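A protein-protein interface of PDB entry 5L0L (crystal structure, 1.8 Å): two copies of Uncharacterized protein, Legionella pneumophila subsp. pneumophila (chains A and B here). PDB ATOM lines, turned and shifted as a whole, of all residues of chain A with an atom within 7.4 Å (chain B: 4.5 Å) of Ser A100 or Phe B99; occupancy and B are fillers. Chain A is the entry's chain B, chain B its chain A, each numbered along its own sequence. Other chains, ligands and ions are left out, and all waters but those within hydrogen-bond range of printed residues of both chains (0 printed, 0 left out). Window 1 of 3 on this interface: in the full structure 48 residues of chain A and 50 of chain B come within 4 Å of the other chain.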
ATOM      1  N   ILE A  51      -3.039 -13.626  15.966  1.00  0.00           N
ATOM      2  CA  ILE A  51      -3.602 -14.299  14.799  1.00  0.00           C
ATOM      3  C   ILE A  51      -2.856 -15.590  14.518  1.00  0.00           C
ATOM      4  O   ILE A  51      -1.735 -15.795  15.015  1.00  0.00           O
ATOM      5  CB  ILE A  51      -3.615 -13.420  13.548  1.00  0.00           C
ATOM      6  CG1 ILE A  51      -2.186 -12.973  13.149  1.00  0.00           C
ATOM      7  CG2 ILE A  51      -4.558 -12.235  13.758  1.00  0.00           C
ATOM      8  CD1 ILE A  51      -2.094 -12.243  11.809  1.00  0.00           C
ATOM      9  N   GLN A  76       6.036 -22.777   2.061  1.00  0.00           N
ATOM     10  CA  GLN A  76       6.669 -21.935   3.096  1.00  0.00           C
ATOM     11  C   GLN A  76       6.782 -20.460   2.701  1.00  0.00           C
ATOM     12  O   GLN A  76       6.496 -19.565   3.503  1.00  0.00           O
ATOM     13  CB  GLN A  76       8.039 -22.481   3.442  1.00  0.00           C
ATOM     14  CG  GLN A  76       8.811 -21.708   4.513  1.00  0.00           C
ATOM     15  CD  GLN A  76       8.222 -21.922   5.885  1.00  0.00           C
ATOM     16  OE1 GLN A  76       8.379 -22.987   6.485  1.00  0.00           O
ATOM     17  NE2 GLN A  76       7.546 -20.929   6.387  1.00  0.00           N
ATOM     18  N   LEU A  79       3.439 -18.718   2.893  1.00  0.00           N
ATOM     19  CA  LEU A  79       3.082 -18.430   4.287  1.00  0.00           C
ATOM     20  C   LEU A  79       3.777 -17.169   4.757  1.00  0.00           C
ATOM     21  O   LEU A  79       3.168 -16.303   5.386  1.00  0.00           O
ATOM     22  CB  LEU A  79       3.461 -19.594   5.190  1.00  0.00           C
ATOM     23  CG  LEU A  79       2.959 -19.475   6.623  1.00  0.00           C
ATOM     24  CD1 LEU A  79       1.523 -19.881   6.703  1.00  0.00           C
ATOM     25  CD2 LEU A  79       3.769 -20.304   7.595  1.00  0.00           C
ATOM     26  N   ASN A  80       5.072 -17.074   4.463  1.00  0.00           N
ATOM     27  CA  ASN A  80       5.856 -15.934   4.897  1.00  0.00           C
ATOM     28  C   ASN A  80       5.474 -14.642   4.172  1.00  0.00           C
ATOM     29  O   ASN A  80       5.606 -13.582   4.743  1.00  0.00           O
ATOM     30  CB  ASN A  80       7.356 -16.250   4.795  1.00  0.00           C
ATOM     31  CG  ASN A  80       7.809 -17.256   5.829  1.00  0.00           C
ATOM     32  OD1 ASN A  80       7.017 -17.855   6.556  1.00  0.00           O
ATOM     33  ND2 ASN A  80       9.103 -17.471   5.893  1.00  0.00           N
ATOM     34  N   ALA A  83       2.378 -13.497   5.948  1.00  0.00           N
ATOM     35  CA  ALA A  83       2.905 -12.895   7.178  1.00  0.00           C
ATOM     36  C   ALA A  83       3.418 -11.479   6.973  1.00  0.00           C
ATOM     37  O   ALA A  83       3.061 -10.564   7.730  1.00  0.00           O
ATOM     38  CB  ALA A  83       3.993 -13.792   7.775  1.00  0.00           C
ATOM     39  N   GLN A  98       5.442  -9.224  16.448  1.00  0.00           N
ATOM     40  CA  GLN A  98       6.242 -10.402  16.715  1.00  0.00           C
ATOM     41  C   GLN A  98       5.553 -11.577  16.034  1.00  0.00           C
ATOM     42  O   GLN A  98       4.341 -11.563  15.853  1.00  0.00           O
ATOM     43  CB  GLN A  98       6.373 -10.636  18.234  1.00  0.00           C
ATOM     44  CG  GLN A  98       7.155  -9.554  18.926  1.00  0.00           C
ATOM     45  CD  GLN A  98       7.513  -9.839  20.366  1.00  0.00           C
ATOM     46  OE1 GLN A  98       6.803 -10.526  21.078  1.00  0.00           O
ATOM     47  NE2 GLN A  98       8.636  -9.273  20.812  1.00  0.00           N
ATOM     48  N   PHE A  99       6.314 -12.602  15.649  1.00  0.00           N
ATOM     49  CA  PHE A  99       5.723 -13.793  15.079  1.00  0.00           C
ATOM     50  C   PHE A  99       6.606 -15.014  15.251  1.00  0.00           C
ATOM     51  O   PHE A  99       7.834 -14.870  15.422  1.00  0.00           O
ATOM     52  CB  PHE A  99       5.309 -13.588  13.603  1.00  0.00           C
ATOM     53  CG  PHE A  99       6.425 -13.181  12.672  1.00  0.00           C
ATOM     54  CD1 PHE A  99       7.263 -14.132  12.126  1.00  0.00           C
ATOM     55  CD2 PHE A  99       6.575 -11.859  12.269  1.00  0.00           C
ATOM     56  CE1 PHE A  99       8.272 -13.780  11.222  1.00  0.00           C
ATOM     57  CE2 PHE A  99       7.554 -11.510  11.359  1.00  0.00           C
ATOM     58  CZ  PHE A  99       8.417 -12.471  10.854  1.00  0.00           C
ATOM     59  N   SER A 100       5.968 -16.189  15.287  1.00  0.00           N
ATOM     60  CA  SER A 100       6.673 -17.471  15.426  1.00  0.00           C
ATOM     61  C   SER A 100       6.030 -18.557  14.633  1.00  0.00           C
ATOM     62  O   SER A 100       4.795 -18.745  14.675  1.00  0.00           O
ATOM     63  CB  SER A 100       6.718 -17.956  16.885  1.00  0.00           C
ATOM     64  OG  SER A 100       7.456 -17.061  17.716  1.00  0.00           O
ATOM     65  N   GLN A 101       6.870 -19.320  13.934  1.00  0.00           N
ATOM     66  CA  GLN A 101       6.471 -20.601  13.352  1.00  0.00           C
ATOM     67  C   GLN A 101       7.068 -21.685  14.245  1.00  0.00           C
ATOM     68  O   GLN A 101       8.310 -21.805  14.344  1.00  0.00           O
ATOM     69  CB  GLN A 101       6.964 -20.763  11.911  1.00  0.00           C
ATOM     70  CG  GLN A 101       6.604 -22.125  11.298  1.00  0.00           C
ATOM     71  CD  GLN A 101       6.926 -22.174   9.811  1.00  0.00           C
ATOM     72  OE1 GLN A 101       6.521 -21.301   9.059  1.00  0.00           O
ATOM     73  NE2 GLN A 101       7.705 -23.132   9.412  1.00  0.00           N
ATOM     74  N   LEU A 102       6.192 -22.450  14.909  1.00  0.00           N
ATOM     75  CA  LEU A 102       6.624 -23.418  15.930  1.00  0.00           C
ATOM     76  C   LEU A 102       6.110 -24.808  15.590  1.00  0.00           C
ATOM     77  O   LEU A 102       6.860 -25.633  15.039  1.00  0.00           O
ATOM     78  CB  LEU A 102       6.218 -22.968  17.349  1.00  0.00           C
ATOM     79  CG  LEU A 102       6.727 -21.599  17.795  1.00  0.00           C
ATOM     80  CD1 LEU A 102       6.268 -21.260  19.213  1.00  0.00           C
ATOM     81  CD2 LEU A 102       8.238 -21.518  17.669  1.00  0.00           C
ATOM     82  N   GLY A 103       4.843 -25.075  15.875  1.00  0.00           N
ATOM     83  CA  GLY A 103       4.312 -26.433  15.657  1.00  0.00           C
ATOM     84  C   GLY A 103       4.502 -27.384  16.832  1.00  0.00           C
ATOM     85  O   GLY A 103       4.271 -28.589  16.678  1.00  0.00           O
ATOM     86  N   LEU A 127       0.973 -26.421   8.208  1.00  0.00           N
ATOM     87  CA  LEU A 127       1.922 -25.330   8.034  1.00  0.00           C
ATOM     88  C   LEU A 127       1.230 -24.059   8.526  1.00  0.00           C
ATOM     89  O   LEU A 127       0.207 -23.615   7.962  1.00  0.00           O
ATOM     90  CB  LEU A 127       2.376 -25.183   6.577  1.00  0.00           C
ATOM     91  CG  LEU A 127       3.272 -23.994   6.232  1.00  0.00           C
ATOM     92  CD1 LEU A 127       4.598 -24.061   7.014  1.00  0.00           C
ATOM     93  CD2 LEU A 127       3.513 -23.917   4.744  1.00  0.00           C
ATOM     94  N   HIS A 128       1.750 -23.483   9.600  1.00  0.00           N
ATOM     95  CA  HIS A 128       1.085 -22.290  10.163  1.00  0.00           C
ATOM     96  C   HIS A 128       2.014 -21.509  11.034  1.00  0.00           C
ATOM     97  O   HIS A 128       2.989 -22.080  11.542  1.00  0.00           O
ATOM     98  CB  HIS A 128      -0.181 -22.681  10.948  1.00  0.00           C
ATOM     99  CG  HIS A 128       0.086 -23.356  12.259  1.00  0.00           C
ATOM    100  ND1 HIS A 128       0.645 -24.607  12.350  1.00  0.00           N
ATOM    101  CD2 HIS A 128      -0.107 -22.944  13.534  1.00  0.00           C
ATOM    102  CE1 HIS A 128       0.751 -24.964  13.621  1.00  0.00           C
ATOM    103  NE2 HIS A 128       0.312 -23.968  14.361  1.00  0.00           N
ATOM    104  N   LEU A 129       1.720 -20.213  11.210  1.00  0.00           N
ATOM    105  CA  LEU A 129       2.450 -19.428  12.184  1.00  0.00           C
ATOM    106  C   LEU A 129       1.561 -18.484  12.971  1.00  0.00           C
ATOM    107  O   LEU A 129       0.409 -18.252  12.617  1.00  0.00           O
ATOM    108  CB  LEU A 129       3.644 -18.687  11.556  1.00  0.00           C
ATOM    109  CG  LEU A 129       3.419 -17.622  10.487  1.00  0.00           C
ATOM    110  CD1 LEU A 129       2.898 -16.324  11.067  1.00  0.00           C
ATOM    111  CD2 LEU A 129       4.731 -17.354   9.754  1.00  0.00           C
ATOM    112  N   HIS A 130       2.133 -17.965  14.041  1.00  0.00           N
ATOM    113  CA  HIS A 130       1.446 -17.104  15.011  1.00  0.00           C
ATOM    114  C   HIS A 130       2.031 -15.710  14.875  1.00  0.00           C
ATOM    115  O   HIS A 130       3.231 -15.594  14.687  1.00  0.00           O
ATOM    116  CB  HIS A 130       1.715 -17.600  16.451  1.00  0.00           C
ATOM    117  CG  HIS A 130       1.278 -19.006  16.690  1.00  0.00           C
ATOM    118  ND1 HIS A 130      -0.025 -19.340  16.951  1.00  0.00           N
ATOM    119  CD2 HIS A 130       1.954 -20.170  16.603  1.00  0.00           C
ATOM    120  CE1 HIS A 130      -0.124 -20.656  17.073  1.00  0.00           C
ATOM    121  NE2 HIS A 130       1.063 -21.186  16.849  1.00  0.00           N
ATOM    122  N   MET A 131       1.183 -14.678  14.983  1.00  0.00           N
ATOM    123  CA  MET A 131       1.636 -13.284  14.995  1.00  0.00           C
ATOM    124  C   MET A 131       0.848 -12.544  16.055  1.00  0.00           C
ATOM    125  O   MET A 131      -0.313 -12.896  16.349  1.00  0.00           O
ATOM    126  CB  MET A 131       1.452 -12.678  13.615  1.00  0.00           C
ATOM    127  CG  MET A 131       1.941 -11.249  13.516  1.00  0.00           C
ATOM    128  SD  MET A 131       1.810 -10.596  11.648  1.00  0.00           S
ATOM    129  CE  MET A 131       3.054 -11.817  10.806  1.00  0.00           C
ATOM    130  N   TRP A 132       1.484 -11.561  16.664  1.00  0.00           N
ATOM    131  CA  TRP A 132       0.835 -10.784  17.696  1.00  0.00           C
ATOM    132  C   TRP A 132       1.517  -9.435  17.828  1.00  0.00           C
ATOM    133  O   TRP A 132       2.584  -9.196  17.237  1.00  0.00           O
ATOM    134  CB  TRP A 132       0.841 -11.558  19.037  1.00  0.00           C
ATOM    135  CG  TRP A 132       2.202 -11.836  19.537  1.00  0.00           C
ATOM    136  CD1 TRP A 132       2.914 -11.088  20.424  1.00  0.00           C
ATOM    137  CD2 TRP A 132       3.046 -12.937  19.155  1.00  0.00           C
ATOM    138  NE1 TRP A 132       4.161 -11.669  20.630  1.00  0.00           N
ATOM    139  CE2 TRP A 132       4.257 -12.793  19.843  1.00  0.00           C
ATOM    140  CE3 TRP A 132       2.882 -14.028  18.286  1.00  0.00           C
ATOM    141  CZ2 TRP A 132       5.330 -13.676  19.678  1.00  0.00           C
ATOM    142  CZ3 TRP A 132       3.935 -14.882  18.091  1.00  0.00           C
ATOM    143  CH2 TRP A 132       5.169 -14.698  18.776  1.00  0.00           C
ATOM    144  N   MET A 155       9.476 -11.963  27.445  1.00  0.00           N
ATOM    145  CA  MET A 155       9.110 -12.965  26.447  1.00  0.00           C
ATOM    146  C   MET A 155       7.618 -13.223  26.517  1.00  0.00           C
ATOM    147  O   MET A 155       7.086 -13.524  27.589  1.00  0.00           O
ATOM    148  CB  MET A 155       9.881 -14.246  26.759  1.00  0.00           C
ATOM    149  CG  MET A 155       9.536 -15.400  25.818  1.00  0.00           C
ATOM    150  SD  MET A 155      10.496 -15.108  24.122  1.00  0.00           S
ATOM    151  CE  MET A 155      12.288 -15.465  24.798  1.00  0.00           C
ATOM    152  N   PHE A 156       6.961 -13.183  25.366  1.00  0.00           N
ATOM    153  CA  PHE A 156       5.549 -13.614  25.209  1.00  0.00           C
ATOM    154  C   PHE A 156       5.524 -15.140  25.061  1.00  0.00           C
ATOM    155  O   PHE A 156       6.148 -15.685  24.132  1.00  0.00           O
ATOM    156  CB  PHE A 156       4.961 -12.913  23.964  1.00  0.00           C
ATOM    157  CG  PHE A 156       3.456 -12.985  23.830  1.00  0.00           C
ATOM    158  CD1 PHE A 156       2.818 -14.188  23.575  1.00  0.00           C
ATOM    159  CD2 PHE A 156       2.684 -11.855  23.949  1.00  0.00           C
ATOM    160  CE1 PHE A 156       1.425 -14.253  23.443  1.00  0.00           C
ATOM    161  CE2 PHE A 156       1.295 -11.901  23.797  1.00  0.00           C
ATOM    162  CZ  PHE A 156       0.668 -13.095  23.526  1.00  0.00           C
ATOM    163  N   LEU A 158       3.715 -18.332  24.021  1.00  0.00           N
ATOM    164  CA  LEU A 158       2.581 -18.750  23.167  1.00  0.00           C
ATOM    165  C   LEU A 158       1.824 -19.987  23.680  1.00  0.00           C
ATOM    166  O   LEU A 158       0.727 -20.279  23.172  1.00  0.00           O
ATOM    167  CB  LEU A 158       3.016 -19.017  21.726  1.00  0.00           C
ATOM    168  CG  LEU A 158       3.515 -17.777  20.988  1.00  0.00           C
ATOM    169  CD1 LEU A 158       4.166 -18.166  19.675  1.00  0.00           C
ATOM    170  CD2 LEU A 158       2.398 -16.766  20.731  1.00  0.00           C
ATOM    171  N   THR B  87      14.950 -21.777   5.575  1.00  0.00           N
ATOM    172  CA  THR B  87      14.229 -22.969   6.031  1.00  0.00           C
ATOM    173  C   THR B  87      14.649 -24.266   5.298  1.00  0.00           C
ATOM    174  O   THR B  87      14.643 -25.348   5.896  1.00  0.00           O
ATOM    175  CB  THR B  87      12.697 -22.869   5.918  1.00  0.00           C
ATOM    176  OG1 THR B  87      12.311 -22.789   4.535  1.00  0.00           O
ATOM    177  CG2 THR B  87      12.143 -21.664   6.728  1.00  0.00           C
ATOM    178  N   GLN B  98      11.917 -24.047  12.985  1.00  0.00           N
ATOM    179  CA  GLN B  98      11.153 -23.060  13.750  1.00  0.00           C
ATOM    180  C   GLN B  98      11.827 -21.709  13.603  1.00  0.00           C
ATOM    181  O   GLN B  98      13.055 -21.615  13.382  1.00  0.00           O
ATOM    182  CB  GLN B  98      11.055 -23.446  15.231  1.00  0.00           C
ATOM    183  CG  GLN B  98      10.301 -24.761  15.420  1.00  0.00           C
ATOM    184  CD  GLN B  98      10.035 -25.112  16.873  1.00  0.00           C
ATOM    185  OE1 GLN B  98      10.786 -24.740  17.785  1.00  0.00           O
ATOM    186  NE2 GLN B  98       8.955 -25.845  17.090  1.00  0.00           N
ATOM    187  N   PHE B  99      11.047 -20.636  13.694  1.00  0.00           N
ATOM    188  CA  PHE B  99      11.617 -19.301  13.676  1.00  0.00           C
ATOM    189  C   PHE B  99      10.749 -18.288  14.415  1.00  0.00           C
ATOM    190  O   PHE B  99       9.523 -18.495  14.547  1.00  0.00           O
ATOM    191  CB  PHE B  99      11.949 -18.801  12.226  1.00  0.00           C
ATOM    192  CG  PHE B  99      10.792 -18.794  11.260  1.00  0.00           C
ATOM    193  CD1 PHE B  99       9.929 -17.704  11.181  1.00  0.00           C
ATOM    194  CD2 PHE B  99      10.586 -19.855  10.398  1.00  0.00           C
ATOM    195  CE1 PHE B  99       8.881 -17.695  10.291  1.00  0.00           C
ATOM    196  CE2 PHE B  99       9.534 -19.852   9.493  1.00  0.00           C
ATOM    197  CZ  PHE B  99       8.681 -18.775   9.452  1.00  0.00           C
ATOM    198  N   SER B 100      11.383 -17.212  14.885  1.00  0.00           N
ATOM    199  CA  SER B 100      10.677 -16.146  15.608  1.00  0.00           C
ATOM    200  C   SER B 100      11.305 -14.793  15.311  1.00  0.00           C
ATOM    201  O   SER B 100      12.545 -14.651  15.363  1.00  0.00           O
ATOM    202  CB  SER B 100      10.728 -16.343  17.129  1.00  0.00           C
ATOM    203  OG  SER B 100      10.093 -17.515  17.615  1.00  0.00           O
ATOM    204  N   LEU B 102      11.235 -11.369  17.220  1.00  0.00           N
ATOM    205  CA  LEU B 102      10.881 -10.942  18.570  1.00  0.00           C
ATOM    206  C   LEU B 102      11.381  -9.530  18.803  1.00  0.00           C
ATOM    207  O   LEU B 102      10.610  -8.583  18.685  1.00  0.00           O
ATOM    208  CB  LEU B 102      11.379 -11.944  19.621  1.00  0.00           C
ATOM    209  CG  LEU B 102      10.884 -13.375  19.514  1.00  0.00           C
ATOM    210  CD1 LEU B 102      11.396 -14.221  20.693  1.00  0.00           C
ATOM    211  CD2 LEU B 102       9.375 -13.521  19.437  1.00  0.00           C
ATOM    212  N   LEU B 129      15.458 -11.811  12.707  1.00  0.00           N
ATOM    213  CA  LEU B 129      14.741 -12.918  13.282  1.00  0.00           C
ATOM    214  C   LEU B 129      15.682 -14.084  13.543  1.00  0.00           C
ATOM    215  O   LEU B 129      16.811 -14.108  13.057  1.00  0.00           O
ATOM    216  CB  LEU B 129      13.544 -13.343  12.442  1.00  0.00           C
ATOM    217  CG  LEU B 129      13.695 -13.884  11.026  1.00  0.00           C
ATOM    218  CD1 LEU B 129      14.173 -15.327  11.000  1.00  0.00           C
ATOM    219  CD2 LEU B 129      12.361 -13.777  10.298  1.00  0.00           C
ATOM    220  N   HIS B 130      15.181 -15.013  14.339  1.00  0.00           N
ATOM    221  CA  HIS B 130      15.928 -16.190  14.808  1.00  0.00           C
ATOM    222  C   HIS B 130      15.323 -17.403  14.140  1.00  0.00           C
ATOM    223  O   HIS B 130      14.115 -17.487  13.994  1.00  0.00           O
ATOM    224  CB  HIS B 130      15.759 -16.358  16.317  1.00  0.00           C
ATOM    225  CG  HIS B 130      16.188 -15.167  17.090  1.00  0.00           C
ATOM    226  ND1 HIS B 130      17.504 -14.939  17.404  1.00  0.00           N
ATOM    227  CD2 HIS B 130      15.491 -14.094  17.536  1.00  0.00           C
ATOM    228  CE1 HIS B 130      17.601 -13.770  18.025  1.00  0.00           C
ATOM    229  NE2 HIS B 130      16.384 -13.263  18.159  1.00  0.00           N
ATOM    230  N   MET B 131      16.162 -18.364  13.787  1.00  0.00           N
ATOM    231  CA  MET B 131      15.694 -19.627  13.196  1.00  0.00           C
ATOM    232  C   MET B 131      16.550 -20.757  13.772  1.00  0.00           C
ATOM    233  O   MET B 131      17.741 -20.550  14.102  1.00  0.00           O
ATOM    234  CB  MET B 131      15.786 -19.553  11.668  1.00  0.00           C
ATOM    235  CG  MET B 131      15.293 -20.817  11.017  1.00  0.00           C
ATOM    236  SD  MET B 131      15.298 -20.706   9.037  1.00  0.00           S
ATOM    237  CE  MET B 131      14.007 -19.256   8.829  1.00  0.00           C
ATOM    238  N   TRP B 132      15.943 -21.923  13.963  1.00  0.00           N
ATOM    239  CA  TRP B 132      16.654 -23.064  14.544  1.00  0.00           C
ATOM    240  C   TRP B 132      15.942 -24.337  14.152  1.00  0.00           C
ATOM    241  O   TRP B 132      14.856 -24.293  13.521  1.00  0.00           O
ATOM    242  CB  TRP B 132      16.743 -22.924  16.084  1.00  0.00           C
ATOM    243  CG  TRP B 132      15.392 -22.884  16.720  1.00  0.00           C
ATOM    244  CD1 TRP B 132      14.720 -23.930  17.283  1.00  0.00           C
ATOM    245  CD2 TRP B 132      14.525 -21.739  16.845  1.00  0.00           C
ATOM    246  NE1 TRP B 132      13.476 -23.520  17.718  1.00  0.00           N
ATOM    247  CE2 TRP B 132      13.337 -22.184  17.475  1.00  0.00           C
ATOM    248  CE3 TRP B 132      14.631 -20.387  16.484  1.00  0.00           C
ATOM    249  CZ2 TRP B 132      12.272 -21.329  17.771  1.00  0.00           C
ATOM    250  CZ3 TRP B 132      13.552 -19.555  16.727  1.00  0.00           C
ATOM    251  CH2 TRP B 132      12.387 -20.022  17.355  1.00  0.00           C
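O of Leu A102 lies within hydrogen-bond range of NE2 of Gln B98.
O of Phe B99 lies within hydrogen-bond range of N of Gln A101 (2.8 Å).
The side-chain hydroxyl (OG) of Ser A100 sits at hydrogen-bond distance from the side-chain hydroxyl (OG) of Ser B100.
The backbone carbonyl oxygen (O) of Leu B102 sits at hydrogen-bond distance from the side-chain amide nitrogen (NE2) of Gln A98, at 3.0 Å.
Of the 20 printed residues of chain A, 8 touch a printed residue of chain B.
Hydrophobic or aromatic side chains of chain A that line the printed part of chain B: Leu A102 and Met A155.
Hydrophobic or aromatic side chains of chain B that line the printed part of chain A: Phe B99 and Leu B102.
Among the printed residues, 11 pairs touch across the chains.
Phe B99 touches just these residues of chain A: Gln A76 (3.8 Å), Asn A80 (3.5 Å), Ser A100 (3.2 Å) and Gln A101 (2.8 Å).
Of the printed residues of chain B, Gln A76 touches Thr B87 (3.7 Å) and Phe B99 (3.8 Å).
Printed residues of chain A within 4 Å of Thr B87: Gln A76 (3.7 Å).
Printed residues of chain B within 4 Å of Asn A80: Phe B99.
Phe A156 touches none of the printed residues of chain B.
The nearest printed residue of chain A that does not touch Thr B87 is Asn A80 (5.2 Å).
Among the printed residues, merely in contact across the chains: Phe A99 with Ser B100 (3.1 Å), Ser A100 with Phe B99 (3.2 Å), Gln A101 with Gln B98 (3.2 Å), Asn A80 with Phe B99 (3.5 Å), Met A155 with Leu B102 (3.7 Å), Gln A76 with Thr B87 (3.7 Å) and Gln A76 with Phe B99 (3.8 Å).
Gln A98 touches Leu B102, and with the chains exchanged Leu A102 touches Gln B98.
Phe A99 touches Ser B100, and with the chains exchanged Ser A100 touches Phe B99.
Ser B100 touches its own counterpart, Ser A100.
Positions printed for both chains: 98, 99, 100, 102, 129, 130, 131 and 132.
Of the 11 pairs that touch across the chains among the printed residues, 5 have their exchanged pair printed and touching as well.
The side-chain sulfur (SD) of Met B131 sits at hydrogen-bond distance from the backbone NH (N) of Thr B87, at 3.6 Å.
OE1 of Gln B98 is in hydrogen-bond range of NE1 of Trp B132 (3.0 Å).
The backbone carbonyl oxygen (O) of Ser B100 is in hydrogen-bond range of the backbone NH (N) of His B130, at 2.9 Å.
The side-chain amide nitrogen of Gln A76 sits at hydrogen-bond distance from the side-chain amide oxygen of Asn A80 (3.1 Å).
OE1 of Gln A98 sits at hydrogen-bond distance from NE1 of Trp A132, at 2.9 Å.
The backbone carbonyl oxygen (O) of Ser A100 is in hydrogen-bond range of the backbone NH (N) of His A130, 2.8 Å away.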
